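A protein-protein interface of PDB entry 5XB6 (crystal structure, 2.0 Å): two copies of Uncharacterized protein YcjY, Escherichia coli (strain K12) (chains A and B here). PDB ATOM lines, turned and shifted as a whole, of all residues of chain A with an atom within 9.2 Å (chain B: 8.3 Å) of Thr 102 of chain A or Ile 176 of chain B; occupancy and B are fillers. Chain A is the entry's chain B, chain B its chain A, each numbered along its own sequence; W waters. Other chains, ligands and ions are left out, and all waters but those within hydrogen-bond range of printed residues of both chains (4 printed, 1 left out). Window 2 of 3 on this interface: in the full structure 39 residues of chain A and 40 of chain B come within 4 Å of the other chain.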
ATOM      1  N   PHE A   8     -24.143   9.717 -13.482  1.00  0.00           N
ATOM      2  CA  PHE A   8     -25.051  10.654 -12.838  1.00  0.00           C
ATOM      3  C   PHE A   8     -26.357  10.791 -13.604  1.00  0.00           C
ATOM      4  O   PHE A   8     -26.386  10.656 -14.818  1.00  0.00           O
ATOM      5  CB  PHE A   8     -24.372  12.016 -12.632  1.00  0.00           C
ATOM      6  CG  PHE A   8     -23.821  12.627 -13.894  1.00  0.00           C
ATOM      7  CD1 PHE A   8     -22.511  12.376 -14.287  1.00  0.00           C
ATOM      8  CD2 PHE A   8     -24.604  13.476 -14.675  1.00  0.00           C
ATOM      9  CE1 PHE A   8     -21.993  12.934 -15.443  1.00  0.00           C
ATOM     10  CE2 PHE A   8     -24.089  14.046 -15.842  1.00  0.00           C
ATOM     11  CZ  PHE A   8     -22.780  13.770 -16.225  1.00  0.00           C
ATOM     12  N   THR A   9     -27.436  11.043 -12.874  1.00  0.00           N
ATOM     13  CA  THR A   9     -28.755  11.263 -13.451  1.00  0.00           C
ATOM     14  C   THR A   9     -28.726  12.393 -14.484  1.00  0.00           C
ATOM     15  O   THR A   9     -28.233  13.485 -14.199  1.00  0.00           O
ATOM     16  CB  THR A   9     -29.751  11.653 -12.333  1.00  0.00           C
ATOM     17  OG1 THR A   9     -29.732  10.653 -11.308  1.00  0.00           O
ATOM     18  CG2 THR A   9     -31.158  11.787 -12.877  1.00  0.00           C
ATOM     19  N   ASN A  10     -29.243  12.129 -15.681  1.00  0.00           N
ATOM     20  CA  ASN A  10     -29.420  13.173 -16.697  1.00  0.00           C
ATOM     21  C   ASN A  10     -30.581  14.030 -16.234  1.00  0.00           C
ATOM     22  O   ASN A  10     -31.722  13.573 -16.187  1.00  0.00           O
ATOM     23  CB  ASN A  10     -29.746  12.550 -18.068  1.00  0.00           C
ATOM     24  CG  ASN A  10     -29.755  13.577 -19.204  1.00  0.00           C
ATOM     25  OD1 ASN A  10     -30.307  14.666 -19.064  1.00  0.00           O
ATOM     26  ND2 ASN A  10     -29.130  13.228 -20.339  1.00  0.00           N
ATOM     27  N   SER A  11     -30.298  15.272 -15.887  1.00  0.00           N
ATOM     28  CA  SER A  11     -31.342  16.170 -15.407  1.00  0.00           C
ATOM     29  C   SER A  11     -32.450  16.441 -16.429  1.00  0.00           C
ATOM     30  O   SER A  11     -33.555  16.819 -16.033  1.00  0.00           O
ATOM     31  CB  SER A  11     -30.737  17.501 -14.949  1.00  0.00           C
ATOM     32  OG  SER A  11     -30.254  18.251 -16.041  1.00  0.00           O
ATOM     33  N   ASN A  12     -32.169  16.284 -17.731  1.00  0.00           N
ATOM     34  CA  ASN A  12     -33.211  16.494 -18.749  1.00  0.00           C
ATOM     35  C   ASN A  12     -34.153  15.304 -18.838  1.00  0.00           C
ATOM     36  O   ASN A  12     -35.299  15.433 -19.274  1.00  0.00           O
ATOM     37  CB  ASN A  12     -32.621  16.724 -20.148  1.00  0.00           C
ATOM     38  CG  ASN A  12     -31.459  17.687 -20.151  1.00  0.00           C
ATOM     39  OD1 ASN A  12     -31.493  18.722 -19.483  1.00  0.00           O
ATOM     40  ND2 ASN A  12     -30.417  17.357 -20.926  1.00  0.00           N
ATOM     41  N   ILE A  22     -14.047  12.013 -15.444  1.00  0.00           N
ATOM     42  CA  ILE A  22     -13.466  13.300 -15.063  1.00  0.00           C
ATOM     43  C   ILE A  22     -11.940  13.180 -15.014  1.00  0.00           C
ATOM     44  O   ILE A  22     -11.399  12.261 -14.399  1.00  0.00           O
ATOM     45  CB  ILE A  22     -13.965  13.771 -13.677  1.00  0.00           C
ATOM     46  CG1 ILE A  22     -15.490  13.756 -13.607  1.00  0.00           C
ATOM     47  CG2 ILE A  22     -13.439  15.171 -13.358  1.00  0.00           C
ATOM     48  CD1 ILE A  22     -16.045  14.083 -12.218  1.00  0.00           C
ATOM     49  N   ILE A  66     -14.217  16.785 -18.579  1.00  0.00           N
ATOM     50  CA  ILE A  66     -15.134  15.662 -18.479  1.00  0.00           C
ATOM     51  C   ILE A  66     -15.514  15.160 -19.863  1.00  0.00           C
ATOM     52  O   ILE A  66     -15.965  15.935 -20.722  1.00  0.00           O
ATOM     53  CB  ILE A  66     -16.371  15.999 -17.588  1.00  0.00           C
ATOM     54  CG1 ILE A  66     -17.228  14.759 -17.327  1.00  0.00           C
ATOM     55  CG2 ILE A  66     -17.183  17.188 -18.150  1.00  0.00           C
ATOM     56  CD1 ILE A  66     -18.272  14.984 -16.223  1.00  0.00           C
ATOM     57  N   SER A  94     -25.854  20.296 -21.631  1.00  0.00           N
ATOM     58  CA  SER A  94     -26.416  21.049 -20.506  1.00  0.00           C
ATOM     59  C   SER A  94     -26.572  20.162 -19.293  1.00  0.00           C
ATOM     60  O   SER A  94     -26.393  20.615 -18.158  1.00  0.00           O
ATOM     61  CB  SER A  94     -27.778  21.666 -20.864  1.00  0.00           C
ATOM     62  OG  SER A  94     -27.602  22.675 -21.830  1.00  0.00           O
ATOM     63  N   ALA A  95     -26.930  18.901 -19.517  1.00  0.00           N
ATOM     64  CA  ALA A  95     -27.041  17.989 -18.369  1.00  0.00           C
ATOM     65  C   ALA A  95     -25.670  17.751 -17.689  1.00  0.00           C
ATOM     66  O   ALA A  95     -25.546  17.684 -16.440  1.00  0.00           O
ATOM     67  CB  ALA A  95     -27.692  16.671 -18.788  1.00  0.00           C
ATOM     68  N   VAL A  96     -24.640  17.634 -18.522  1.00  0.00           N
ATOM     69  CA  VAL A  96     -23.270  17.477 -18.042  1.00  0.00           C
ATOM     70  C   VAL A  96     -22.862  18.729 -17.237  1.00  0.00           C
ATOM     71  O   VAL A  96     -22.335  18.613 -16.125  1.00  0.00           O
ATOM     72  CB  VAL A  96     -22.313  17.170 -19.225  1.00  0.00           C
ATOM     73  CG1 VAL A  96     -20.873  17.060 -18.757  1.00  0.00           C
ATOM     74  CG2 VAL A  96     -22.751  15.856 -19.926  1.00  0.00           C
ATOM     75  N   ILE A  97     -23.138  19.917 -17.776  1.00  0.00           N
ATOM     76  CA  ILE A  97     -22.852  21.167 -17.065  1.00  0.00           C
ATOM     77  C   ILE A  97     -23.593  21.227 -15.735  1.00  0.00           C
ATOM     78  O   ILE A  97     -23.025  21.629 -14.709  1.00  0.00           O
ATOM     79  CB  ILE A  97     -23.180  22.400 -17.934  1.00  0.00           C
ATOM     80  CG1 ILE A  97     -22.151  22.523 -19.057  1.00  0.00           C
ATOM     81  CG2 ILE A  97     -23.186  23.700 -17.099  1.00  0.00           C
ATOM     82  CD1 ILE A  97     -22.582  23.448 -20.167  1.00  0.00           C
ATOM     83  N   ASP A  98     -24.852  20.803 -15.735  1.00  0.00           N
ATOM     84  CA  ASP A  98     -25.615  20.720 -14.491  1.00  0.00           C
ATOM     85  C   ASP A  98     -24.842  19.892 -13.476  1.00  0.00           C
ATOM     86  O   ASP A  98     -24.677  20.310 -12.328  1.00  0.00           O
ATOM     87  CB  ASP A  98     -26.973  20.050 -14.716  1.00  0.00           C
ATOM     88  CG  ASP A  98     -27.952  20.927 -15.467  1.00  0.00           C
ATOM     89  OD1 ASP A  98     -27.684  22.145 -15.633  1.00  0.00           O
ATOM     90  OD2 ASP A  98     -29.011  20.381 -15.863  1.00  0.00           O
ATOM     91  N   TYR A  99     -24.363  18.722 -13.906  1.00  0.00           N
ATOM     92  CA  TYR A  99     -23.547  17.893 -13.016  1.00  0.00           C
ATOM     93  C   TYR A  99     -22.298  18.622 -12.524  1.00  0.00           C
ATOM     94  O   TYR A  99     -21.975  18.557 -11.339  1.00  0.00           O
ATOM     95  CB  TYR A  99     -23.153  16.563 -13.683  1.00  0.00           C
ATOM     96  CG  TYR A  99     -22.187  15.718 -12.872  1.00  0.00           C
ATOM     97  CD1 TYR A  99     -22.624  14.992 -11.767  1.00  0.00           C
ATOM     98  CD2 TYR A  99     -20.840  15.625 -13.233  1.00  0.00           C
ATOM     99  CE1 TYR A  99     -21.749  14.201 -11.034  1.00  0.00           C
ATOM    100  CE2 TYR A  99     -19.956  14.838 -12.509  1.00  0.00           C
ATOM    101  CZ  TYR A  99     -20.418  14.132 -11.410  1.00  0.00           C
ATOM    102  OH  TYR A  99     -19.540  13.356 -10.691  1.00  0.00           O
ATOM    103  N   LEU A 100     -21.605  19.321 -13.422  1.00  0.00           N
ATOM    104  CA  LEU A 100     -20.413  20.065 -13.024  1.00  0.00           C
ATOM    105  C   LEU A 100     -20.732  21.105 -11.950  1.00  0.00           C
ATOM    106  O   LEU A 100     -19.917  21.353 -11.068  1.00  0.00           O
ATOM    107  CB  LEU A 100     -19.738  20.742 -14.217  1.00  0.00           C
ATOM    108  CG  LEU A 100     -19.086  19.811 -15.239  1.00  0.00           C
ATOM    109  CD1 LEU A 100     -18.344  20.614 -16.317  1.00  0.00           C
ATOM    110  CD2 LEU A 100     -18.146  18.839 -14.545  1.00  0.00           C
ATOM    111  N   THR A 101     -21.916  21.708 -11.999  1.00  0.00           N
ATOM    112  CA  THR A 101     -22.209  22.750 -11.012  1.00  0.00           C
ATOM    113  C   THR A 101     -22.357  22.199  -9.604  1.00  0.00           C
ATOM    114  O   THR A 101     -22.362  22.963  -8.647  1.00  0.00           O
ATOM    115  CB  THR A 101     -23.447  23.591 -11.361  1.00  0.00           C
ATOM    116  OG1 THR A 101     -24.632  22.789 -11.231  1.00  0.00           O
ATOM    117  CG2 THR A 101     -23.336  24.134 -12.768  1.00  0.00           C
ATOM    118  N   THR A 102     -22.493  20.883  -9.471  1.00  0.00           N
ATOM    119  CA  THR A 102     -22.649  20.290  -8.150  1.00  0.00           C
ATOM    120  C   THR A 102     -21.301  19.934  -7.563  1.00  0.00           C
ATOM    121  O   THR A 102     -21.223  19.490  -6.423  1.00  0.00           O
ATOM    122  CB  THR A 102     -23.469  19.002  -8.181  1.00  0.00           C
ATOM    123  OG1 THR A 102     -22.713  17.972  -8.835  1.00  0.00           O
ATOM    124  CG2 THR A 102     -24.785  19.224  -8.905  1.00  0.00           C
ATOM    125  N   LEU A 103     -20.250  20.105  -8.357  1.00  0.00           N
ATOM    126  CA  LEU A 103     -18.904  19.757  -7.924  1.00  0.00           C
ATOM    127  C   LEU A 103     -18.190  21.010  -7.425  1.00  0.00           C
ATOM    128  O   LEU A 103     -17.934  21.929  -8.202  1.00  0.00           O
ATOM    129  CB  LEU A 103     -18.114  19.141  -9.081  1.00  0.00           C
ATOM    130  CG  LEU A 103     -18.686  17.914  -9.784  1.00  0.00           C
ATOM    131  CD1 LEU A 103     -17.718  17.445 -10.864  1.00  0.00           C
ATOM    132  CD2 LEU A 103     -18.942  16.801  -8.807  1.00  0.00           C
ATOM    133  N   SER A 104     -17.864  21.040  -6.133  1.00  0.00           N
ATOM    134  CA  SER A 104     -17.299  22.237  -5.496  1.00  0.00           C
ATOM    135  C   SER A 104     -15.994  22.703  -6.119  1.00  0.00           C
ATOM    136  O   SER A 104     -15.671  23.890  -6.083  1.00  0.00           O
ATOM    137  CB  SER A 104     -17.086  21.999  -3.999  1.00  0.00           C
ATOM    138  OG  SER A 104     -16.215  20.908  -3.774  1.00  0.00           O
ATOM    139  N   TYR A 105     -15.241  21.776  -6.698  1.00  0.00           N
ATOM    140  CA  TYR A 105     -13.949  22.141  -7.260  1.00  0.00           C
ATOM    141  C   TYR A 105     -14.015  22.690  -8.683  1.00  0.00           C
ATOM    142  O   TYR A 105     -12.970  22.973  -9.286  1.00  0.00           O
ATOM    143  CB  TYR A 105     -12.970  20.972  -7.184  1.00  0.00           C
ATOM    144  CG  TYR A 105     -13.474  19.708  -7.829  1.00  0.00           C
ATOM    145  CD1 TYR A 105     -13.324  19.501  -9.187  1.00  0.00           C
ATOM    146  CD2 TYR A 105     -14.080  18.716  -7.073  1.00  0.00           C
ATOM    147  CE1 TYR A 105     -13.768  18.343  -9.778  1.00  0.00           C
ATOM    148  CE2 TYR A 105     -14.532  17.563  -7.650  1.00  0.00           C
ATOM    149  CZ  TYR A 105     -14.371  17.381  -9.006  1.00  0.00           C
ATOM    150  OH  TYR A 105     -14.816  16.226  -9.598  1.00  0.00           O
ATOM    151  N   VAL A 106     -15.221  22.828  -9.240  1.00  0.00           N
ATOM    152  CA  VAL A 106     -15.323  23.558 -10.508  1.00  0.00           C
ATOM    153  C   VAL A 106     -15.995  24.923 -10.330  1.00  0.00           C
ATOM    154  O   VAL A 106     -16.948  25.073  -9.555  1.00  0.00           O
ATOM    155  CB  VAL A 106     -15.940  22.716 -11.679  1.00  0.00           C
ATOM    156  CG1 VAL A 106     -16.248  21.288 -11.250  1.00  0.00           C
ATOM    157  CG2 VAL A 106     -17.158  23.394 -12.265  1.00  0.00           C
ATOM    158  N   ASP A 107     -15.443  25.923 -11.006  1.00  0.00           N
ATOM    159  CA  ASP A 107     -15.980  27.272 -10.982  1.00  0.00           C
ATOM    160  C   ASP A 107     -17.108  27.373 -12.001  1.00  0.00           C
ATOM    161  O   ASP A 107     -16.863  27.286 -13.213  1.00  0.00           O
ATOM    162  CB  ASP A 107     -14.873  28.278 -11.330  1.00  0.00           C
ATOM    163  CG  ASP A 107     -15.294  29.725 -11.096  1.00  0.00           C
ATOM    164  OD1 ASP A 107     -16.497  30.034 -11.234  1.00  0.00           O
ATOM    165  OD2 ASP A 107     -14.415  30.562 -10.790  1.00  0.00           O
ATOM    166  N   ASN A 108     -18.337  27.571 -11.519  1.00  0.00           N
ATOM    167  CA  ASN A 108     -19.498  27.660 -12.406  1.00  0.00           C
ATOM    168  C   ASN A 108     -19.352  28.728 -13.486  1.00  0.00           C
ATOM    169  O   ASN A 108     -19.976  28.630 -14.541  1.00  0.00           O
ATOM    170  CB  ASN A 108     -20.780  27.937 -11.618  1.00  0.00           C
ATOM    171  CG  ASN A 108     -21.210  26.769 -10.751  1.00  0.00           C
ATOM    172  OD1 ASN A 108     -20.687  25.664 -10.862  1.00  0.00           O
ATOM    173  ND2 ASN A 108     -22.173  27.020  -9.875  1.00  0.00           N
ATOM    174  N   ILE A 111     -16.753  27.633 -17.269  1.00  0.00           N
ATOM    175  CA  ILE A 111     -16.976  26.358 -17.948  1.00  0.00           C
ATOM    176  C   ILE A 111     -16.973  26.574 -19.446  1.00  0.00           C
ATOM    177  O   ILE A 111     -17.650  27.485 -19.953  1.00  0.00           O
ATOM    178  CB  ILE A 111     -18.317  25.724 -17.530  1.00  0.00           C
ATOM    179  CG1 ILE A 111     -18.291  25.423 -16.034  1.00  0.00           C
ATOM    180  CG2 ILE A 111     -18.601  24.442 -18.351  1.00  0.00           C
ATOM    181  CD1 ILE A 111     -19.631  24.988 -15.434  1.00  0.00           C
ATOM    182  N   ARG A 132     -24.317  29.271 -19.963  1.00  0.00           N
ATOM    183  CA  ARG A 132     -23.281  28.946 -18.991  1.00  0.00           C
ATOM    184  C   ARG A 132     -21.975  28.545 -19.691  1.00  0.00           C
ATOM    185  O   ARG A 132     -20.914  28.500 -19.065  1.00  0.00           O
ATOM    186  CB  ARG A 132     -23.764  27.840 -18.058  1.00  0.00           C
ATOM    187  CG  ARG A 132     -24.987  28.242 -17.241  1.00  0.00           C
ATOM    188  CD  ARG A 132     -25.558  27.058 -16.490  1.00  0.00           C
ATOM    189  NE  ARG A 132     -25.974  25.984 -17.386  1.00  0.00           N
ATOM    190  CZ  ARG A 132     -26.496  24.839 -16.962  1.00  0.00           C
ATOM    191  NH1 ARG A 132     -26.658  24.640 -15.663  1.00  0.00           N
ATOM    192  NH2 ARG A 132     -26.843  23.892 -17.834  1.00  0.00           N
ATOM    193  N   ASN B 170     -29.678  29.431 -16.393  1.00  0.00           N
ATOM    194  CA  ASN B 170     -29.449  29.496 -14.962  1.00  0.00           C
ATOM    195  C   ASN B 170     -30.474  28.689 -14.161  1.00  0.00           C
ATOM    196  O   ASN B 170     -30.179  28.203 -13.072  1.00  0.00           O
ATOM    197  CB  ASN B 170     -29.408  30.968 -14.513  1.00  0.00           C
ATOM    198  CG  ASN B 170     -28.226  31.721 -15.109  1.00  0.00           C
ATOM    199  OD1 ASN B 170     -27.212  31.115 -15.471  1.00  0.00           O
ATOM    200  ND2 ASN B 170     -28.348  33.046 -15.212  1.00  0.00           N
ATOM    201  N   ALA B 171     -31.674  28.524 -14.714  1.00  0.00           N
ATOM    202  CA  ALA B 171     -32.702  27.717 -14.055  1.00  0.00           C
ATOM    203  C   ALA B 171     -32.265  26.257 -13.963  1.00  0.00           C
ATOM    204  O   ALA B 171     -32.660  25.520 -13.050  1.00  0.00           O
ATOM    205  CB  ALA B 171     -34.023  27.825 -14.799  1.00  0.00           C
ATOM    206  N   ARG B 172     -31.481  25.815 -14.935  1.00  0.00           N
ATOM    207  CA  ARG B 172     -31.021  24.436 -14.918  1.00  0.00           C
ATOM    208  C   ARG B 172     -30.067  24.256 -13.738  1.00  0.00           C
ATOM    209  O   ARG B 172     -30.043  23.205 -13.102  1.00  0.00           O
ATOM    210  CB  ARG B 172     -30.353  24.093 -16.257  1.00  0.00           C
ATOM    211  CG  ARG B 172     -31.368  23.805 -17.375  1.00  0.00           C
ATOM    212  CD  ARG B 172     -30.825  24.183 -18.760  1.00  0.00           C
ATOM    213  NE  ARG B 172     -31.891  24.172 -19.752  1.00  0.00           N
ATOM    214  CZ  ARG B 172     -32.264  23.090 -20.426  1.00  0.00           C
ATOM    215  NH1 ARG B 172     -31.625  21.941 -20.230  1.00  0.00           N
ATOM    216  NH2 ARG B 172     -33.270  23.160 -21.300  1.00  0.00           N
ATOM    217  N   THR B 173     -29.282  25.284 -13.465  1.00  0.00           N
ATOM    218  CA  THR B 173     -28.399  25.265 -12.320  1.00  0.00           C
ATOM    219  C   THR B 173     -29.235  25.214 -11.000  1.00  0.00           C
ATOM    220  O   THR B 173     -28.984  24.448 -10.165  1.00  0.00           O
ATOM    221  CB  THR B 173     -27.403  26.461 -12.304  1.00  0.00           C
ATOM    222  OG1 THR B 173     -26.604  26.454 -13.466  1.00  0.00           O
ATOM    223  CG2 THR B 173     -26.531  26.418 -11.070  1.00  0.00           C
ATOM    224  N   SER B 174     -30.249  26.041 -10.897  1.00  0.00           N
ATOM    225  CA  SER B 174     -31.079  26.074  -9.686  1.00  0.00           C
ATOM    226  C   SER B 174     -31.874  24.790  -9.536  1.00  0.00           C
ATOM    227  O   SER B 174     -32.051  24.290  -8.461  1.00  0.00           O
ATOM    228  CB  SER B 174     -31.966  27.288  -9.590  1.00  0.00           C
ATOM    229  OG  SER B 174     -32.036  27.974 -10.779  1.00  0.00           O
ATOM    230  N   ASP B 175     -32.295  24.232 -10.651  1.00  0.00           N
ATOM    231  CA  ASP B 175     -33.070  23.015 -10.594  1.00  0.00           C
ATOM    232  C   ASP B 175     -32.269  21.874  -9.968  1.00  0.00           C
ATOM    233  O   ASP B 175     -32.760  21.145  -9.205  1.00  0.00           O
ATOM    234  CB  ASP B 175     -33.575  22.577 -11.945  1.00  0.00           C
ATOM    235  CG  ASP B 175     -34.722  23.401 -12.465  1.00  0.00           C
ATOM    236  OD1 ASP B 175     -35.151  24.350 -11.864  1.00  0.00           O
ATOM    237  OD2 ASP B 175     -35.129  23.062 -13.527  1.00  0.00           O
ATOM    238  N   ILE B 176     -31.016  21.742 -10.369  1.00  0.00           N
ATOM    239  CA  ILE B 176     -30.238  20.623  -9.845  1.00  0.00           C
ATOM    240  C   ILE B 176     -29.810  20.920  -8.416  1.00  0.00           C
ATOM    241  O   ILE B 176     -29.742  20.021  -7.582  1.00  0.00           O
ATOM    242  CB  ILE B 176     -29.045  20.224 -10.772  1.00  0.00           C
ATOM    243  CG1 ILE B 176     -28.507  18.844 -10.387  1.00  0.00           C
ATOM    244  CG2 ILE B 176     -27.935  21.269 -10.771  1.00  0.00           C
ATOM    245  CD1 ILE B 176     -27.582  18.235 -11.429  1.00  0.00           C
ATOM    246  N   SER B 177     -29.568  22.196  -8.131  1.00  0.00           N
ATOM    247  CA  SER B 177     -29.175  22.614  -6.790  1.00  0.00           C
ATOM    248  C   SER B 177     -30.286  22.362  -5.769  1.00  0.00           C
ATOM    249  O   SER B 177     -30.041  21.799  -4.700  1.00  0.00           O
ATOM    250  CB  SER B 177     -28.752  24.084  -6.796  1.00  0.00           C
ATOM    251  OG  SER B 177     -28.568  24.579  -5.480  1.00  0.00           O
ATOM    252  N   SER B 178     -31.514  22.742  -6.114  1.00  0.00           N
ATOM    253  CA  SER B 178     -32.620  22.679  -5.169  1.00  0.00           C
ATOM    254  C   SER B 178     -33.393  21.371  -5.199  1.00  0.00           C
ATOM    255  O   SER B 178     -34.002  21.000  -4.205  1.00  0.00           O
ATOM    256  CB  SER B 178     -33.592  23.840  -5.396  1.00  0.00           C
ATOM    257  OG  SER B 178     -34.225  23.736  -6.656  1.00  0.00           O
ATOM    258  N   GLY B 179     -33.394  20.678  -6.333  1.00  0.00           N
ATOM    259  CA  GLY B 179     -34.190  19.465  -6.464  1.00  0.00           C
ATOM    260  C   GLY B 179     -35.629  19.785  -6.833  1.00  0.00           C
ATOM    261  O   GLY B 179     -36.484  18.902  -6.890  1.00  0.00           O
ATOM    262  N   GLU B 180     -35.886  21.064  -7.084  1.00  0.00           N
ATOM    263  CA  GLU B 180     -37.200  21.548  -7.487  1.00  0.00           C
ATOM    264  C   GLU B 180     -37.114  21.978  -8.939  1.00  0.00           C
ATOM    265  O   GLU B 180     -36.017  22.152  -9.471  1.00  0.00           O
ATOM    266  CB  GLU B 180     -37.582  22.766  -6.643  1.00  0.00           C
ATOM    267  CG  GLU B 180     -37.781  22.488  -5.166  1.00  0.00           C
ATOM    268  CD  GLU B 180     -39.051  21.717  -4.899  1.00  0.00           C
ATOM    269  OE1 GLU B 180     -40.117  22.356  -4.764  1.00  0.00           O
ATOM    270  OE2 GLU B 180     -38.985  20.470  -4.838  1.00  0.00           O
ATOM    271  N   TYR B 181     -38.257  22.171  -9.586  1.00  0.00           N
ATOM    272  CA  TYR B 181     -38.247  22.685 -10.953  1.00  0.00           C
ATOM    273  C   TYR B 181     -38.854  24.083 -11.004  1.00  0.00           C
ATOM    274  O   TYR B 181     -40.030  24.268 -10.687  1.00  0.00           O
ATOM    275  CB  TYR B 181     -38.974  21.709 -11.899  1.00  0.00           C
ATOM    276  CG  TYR B 181     -38.246  20.385 -12.027  1.00  0.00           C
ATOM    277  CD1 TYR B 181     -37.087  20.279 -12.796  1.00  0.00           C
ATOM    278  CD2 TYR B 181     -38.701  19.247 -11.361  1.00  0.00           C
ATOM    279  CE1 TYR B 181     -36.406  19.058 -12.911  1.00  0.00           C
ATOM    280  CE2 TYR B 181     -38.028  18.031 -11.462  1.00  0.00           C
ATOM    281  CZ  TYR B 181     -36.887  17.946 -12.241  1.00  0.00           C
ATOM    282  OH  TYR B 181     -36.227  16.738 -12.338  1.00  0.00           O
ATOM    283  N   ALA B 182     -38.045  25.071 -11.374  1.00  0.00           N
ATOM    284  CA  ALA B 182     -38.524  26.446 -11.479  1.00  0.00           C
ATOM    285  C   ALA B 182     -39.573  26.508 -12.570  1.00  0.00           C
ATOM    286  O   ALA B 182     -39.445  25.837 -13.601  1.00  0.00           O
ATOM    287  CB  ALA B 182     -37.371  27.420 -11.774  1.00  0.00           C
ATOM    288  N   ARG B 223     -36.717  25.887 -17.080  1.00  0.00           N
ATOM    289  CA  ARG B 223     -35.533  25.313 -17.752  1.00  0.00           C
ATOM    290  C   ARG B 223     -35.693  25.188 -19.276  1.00  0.00           C
ATOM    291  O   ARG B 223     -34.692  25.124 -19.998  1.00  0.00           O
ATOM    292  CB  ARG B 223     -35.217  23.929 -17.176  1.00  0.00           C
ATOM    293  CG  ARG B 223     -36.305  22.900 -17.477  1.00  0.00           C
ATOM    294  CD  ARG B 223     -36.040  21.602 -16.767  1.00  0.00           C
ATOM    295  NE  ARG B 223     -34.869  20.897 -17.308  1.00  0.00           N
ATOM    296  CZ  ARG B 223     -33.753  20.676 -16.620  1.00  0.00           C
ATOM    297  NH1 ARG B 223     -33.657  21.107 -15.369  1.00  0.00           N
ATOM    298  NH2 ARG B 223     -32.734  20.021 -17.176  1.00  0.00           N
HETATM  299  O   HOH W   1     -34.104  16.989 -13.512  1.00  0.00           O
HETATM  300  O   HOH W   2     -30.083  23.402 -22.500  1.00  0.00           O
HETATM  301  O   HOH W   3     -31.027  20.870 -14.081  1.00  0.00           O
HETATM  302  O   HOH W   4     -26.097  23.452  -9.059  1.00  0.00           O
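The guanidinium group (NH2) of Arg 223 of chain B is in hydrogen-bond range of the side-chain amide oxygen (OD1) of Asn 12 of chain A (2.9 Å). The guanidinium group of Arg 223 of chain B is in hydrogen-bond range of the side-chain hydroxyl of Ser 11 of chain A, 3.3 Å away. The guanidinium group (NH2) of Arg 223 of chain B lies within salt-bridge range of the side-chain carboxylate (OD2) of Asp 98 of chain A (3.96 Å). OG1 of Thr 173 of chain B sits at hydrogen-bond distance from NH1 of Arg 132 of chain A (2.8 Å). The side-chain amide oxygen of Asn 12 of chain A lies within hydrogen-bond range of the guanidinium group of Arg 172 of chain B (3.3 Å).
The backbone carbonyl oxygen (O) of Tyr 99 of chain A sits at hydrogen-bond distance from the side-chain hydroxyl (OG1) of Thr 102 of chain A, at 2.7 Å. N of Asn 12 of chain A is in hydrogen-bond range of OD1 of Asn 10 of chain A (2.8 Å). O of Asp 98 of chain A sits at hydrogen-bond distance from OG1 of Thr 101 of chain A, 2.7 Å away. The guanidinium group of Arg 223 of chain B is in salt-bridge range of the side-chain carboxylate of Asp 175 of chain B (3.1 Å).
Ser 94 of chain A touches Arg 172 of chain B. Arg 172 of chain B touches Asp 98 of chain A (CB to OD1, 3.4 Å). Asp 98 of chain A touches Ile 176 of chain B. Ile 176 of chain B touches Thr 101 of chain A. Thr 102 of chain A touches Ile 176 of chain B (CG2 to CD1, 3.9 Å). Arg 172 of chain B touches Arg 132 of chain A (CB to NH1, 3.8 Å).
Thr 102 of chain A touches one residue of chain B. Ile 176 of chain B touches just these residues of chain A: Asp 98 (3.7 Å), Thr 101 (3.7 Å) and Thr 102 (3.9 Å). No residue of chain A comes within 4 Å of Ser 177 of chain B. Of the printed residues of chain B, Thr 101 of chain A touches Ile 176 (3.7 Å). Printed residues of chain B within 4 Å of Asp 98 of chain A: Arg 172, Ile 176 and Arg 223. Of the printed residues of chain B, Arg 132 of chain A touches Arg 172 (3.8 Å) and Thr 173 (2.8 Å). Of the printed residues of chain B, Ser 11 of chain A touches Arg 223. Printed residues of chain A within 4 Å of Arg 223 of chain B: Ser 11, Asn 12 and Asp 98. The nearest residue of chain B that does not touch Thr 102 of chain A is Ser 177 of chain B (5.7 Å). The nearest printed residue of chain A that does not touch Arg 223 of chain B is Ala 95 of chain A (6.2 Å).
Printed residues of chain A that touch a printed residue of chain B: Ser 11, Asn 12, Ser 94, Asp 98, Thr 101, Thr 102 and Arg 132. Of the 14 printed residues of chain B, 4 touch a printed residue of chain A. Hydrophobic or aromatic side chains of chain B within 4 Å of the printed part of chain A: Ile 176. Among the printed residues, Asp or Glu carboxylates within 4 Å of a Lys or Arg side-chain nitrogen of the other chain: Asp 98 of chain A with Arg 223 of chain B.
No position is printed for both chains. Of the 11 pairs that touch across the chains among the printed residues, none has its exchanged pair printed and touching as well.
Water W1 lies within hydrogen-bond range of OH of Tyr 181 of chain B and O of Ser 11 of chain A. Water W2 bridges the side-chain hydroxyl (OG) of Ser 94 of chain A and the guanidinium group (NH1) of Arg 172 of chain B. Water W4 lies within hydrogen-bond range of OG1 of Thr 101 of chain A (2.7 Å) and O of Thr 173 of chain B (3.2 Å). Water W3 lies within hydrogen-bond range of O of Arg 172 of chain B (2.7 Å), OD2 of Asp 98 of chain A (2.7 Å), NH1 of Arg 223 of chain B (2.9 Å) and OG of Ser 11 of chain A (3.4 Å).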
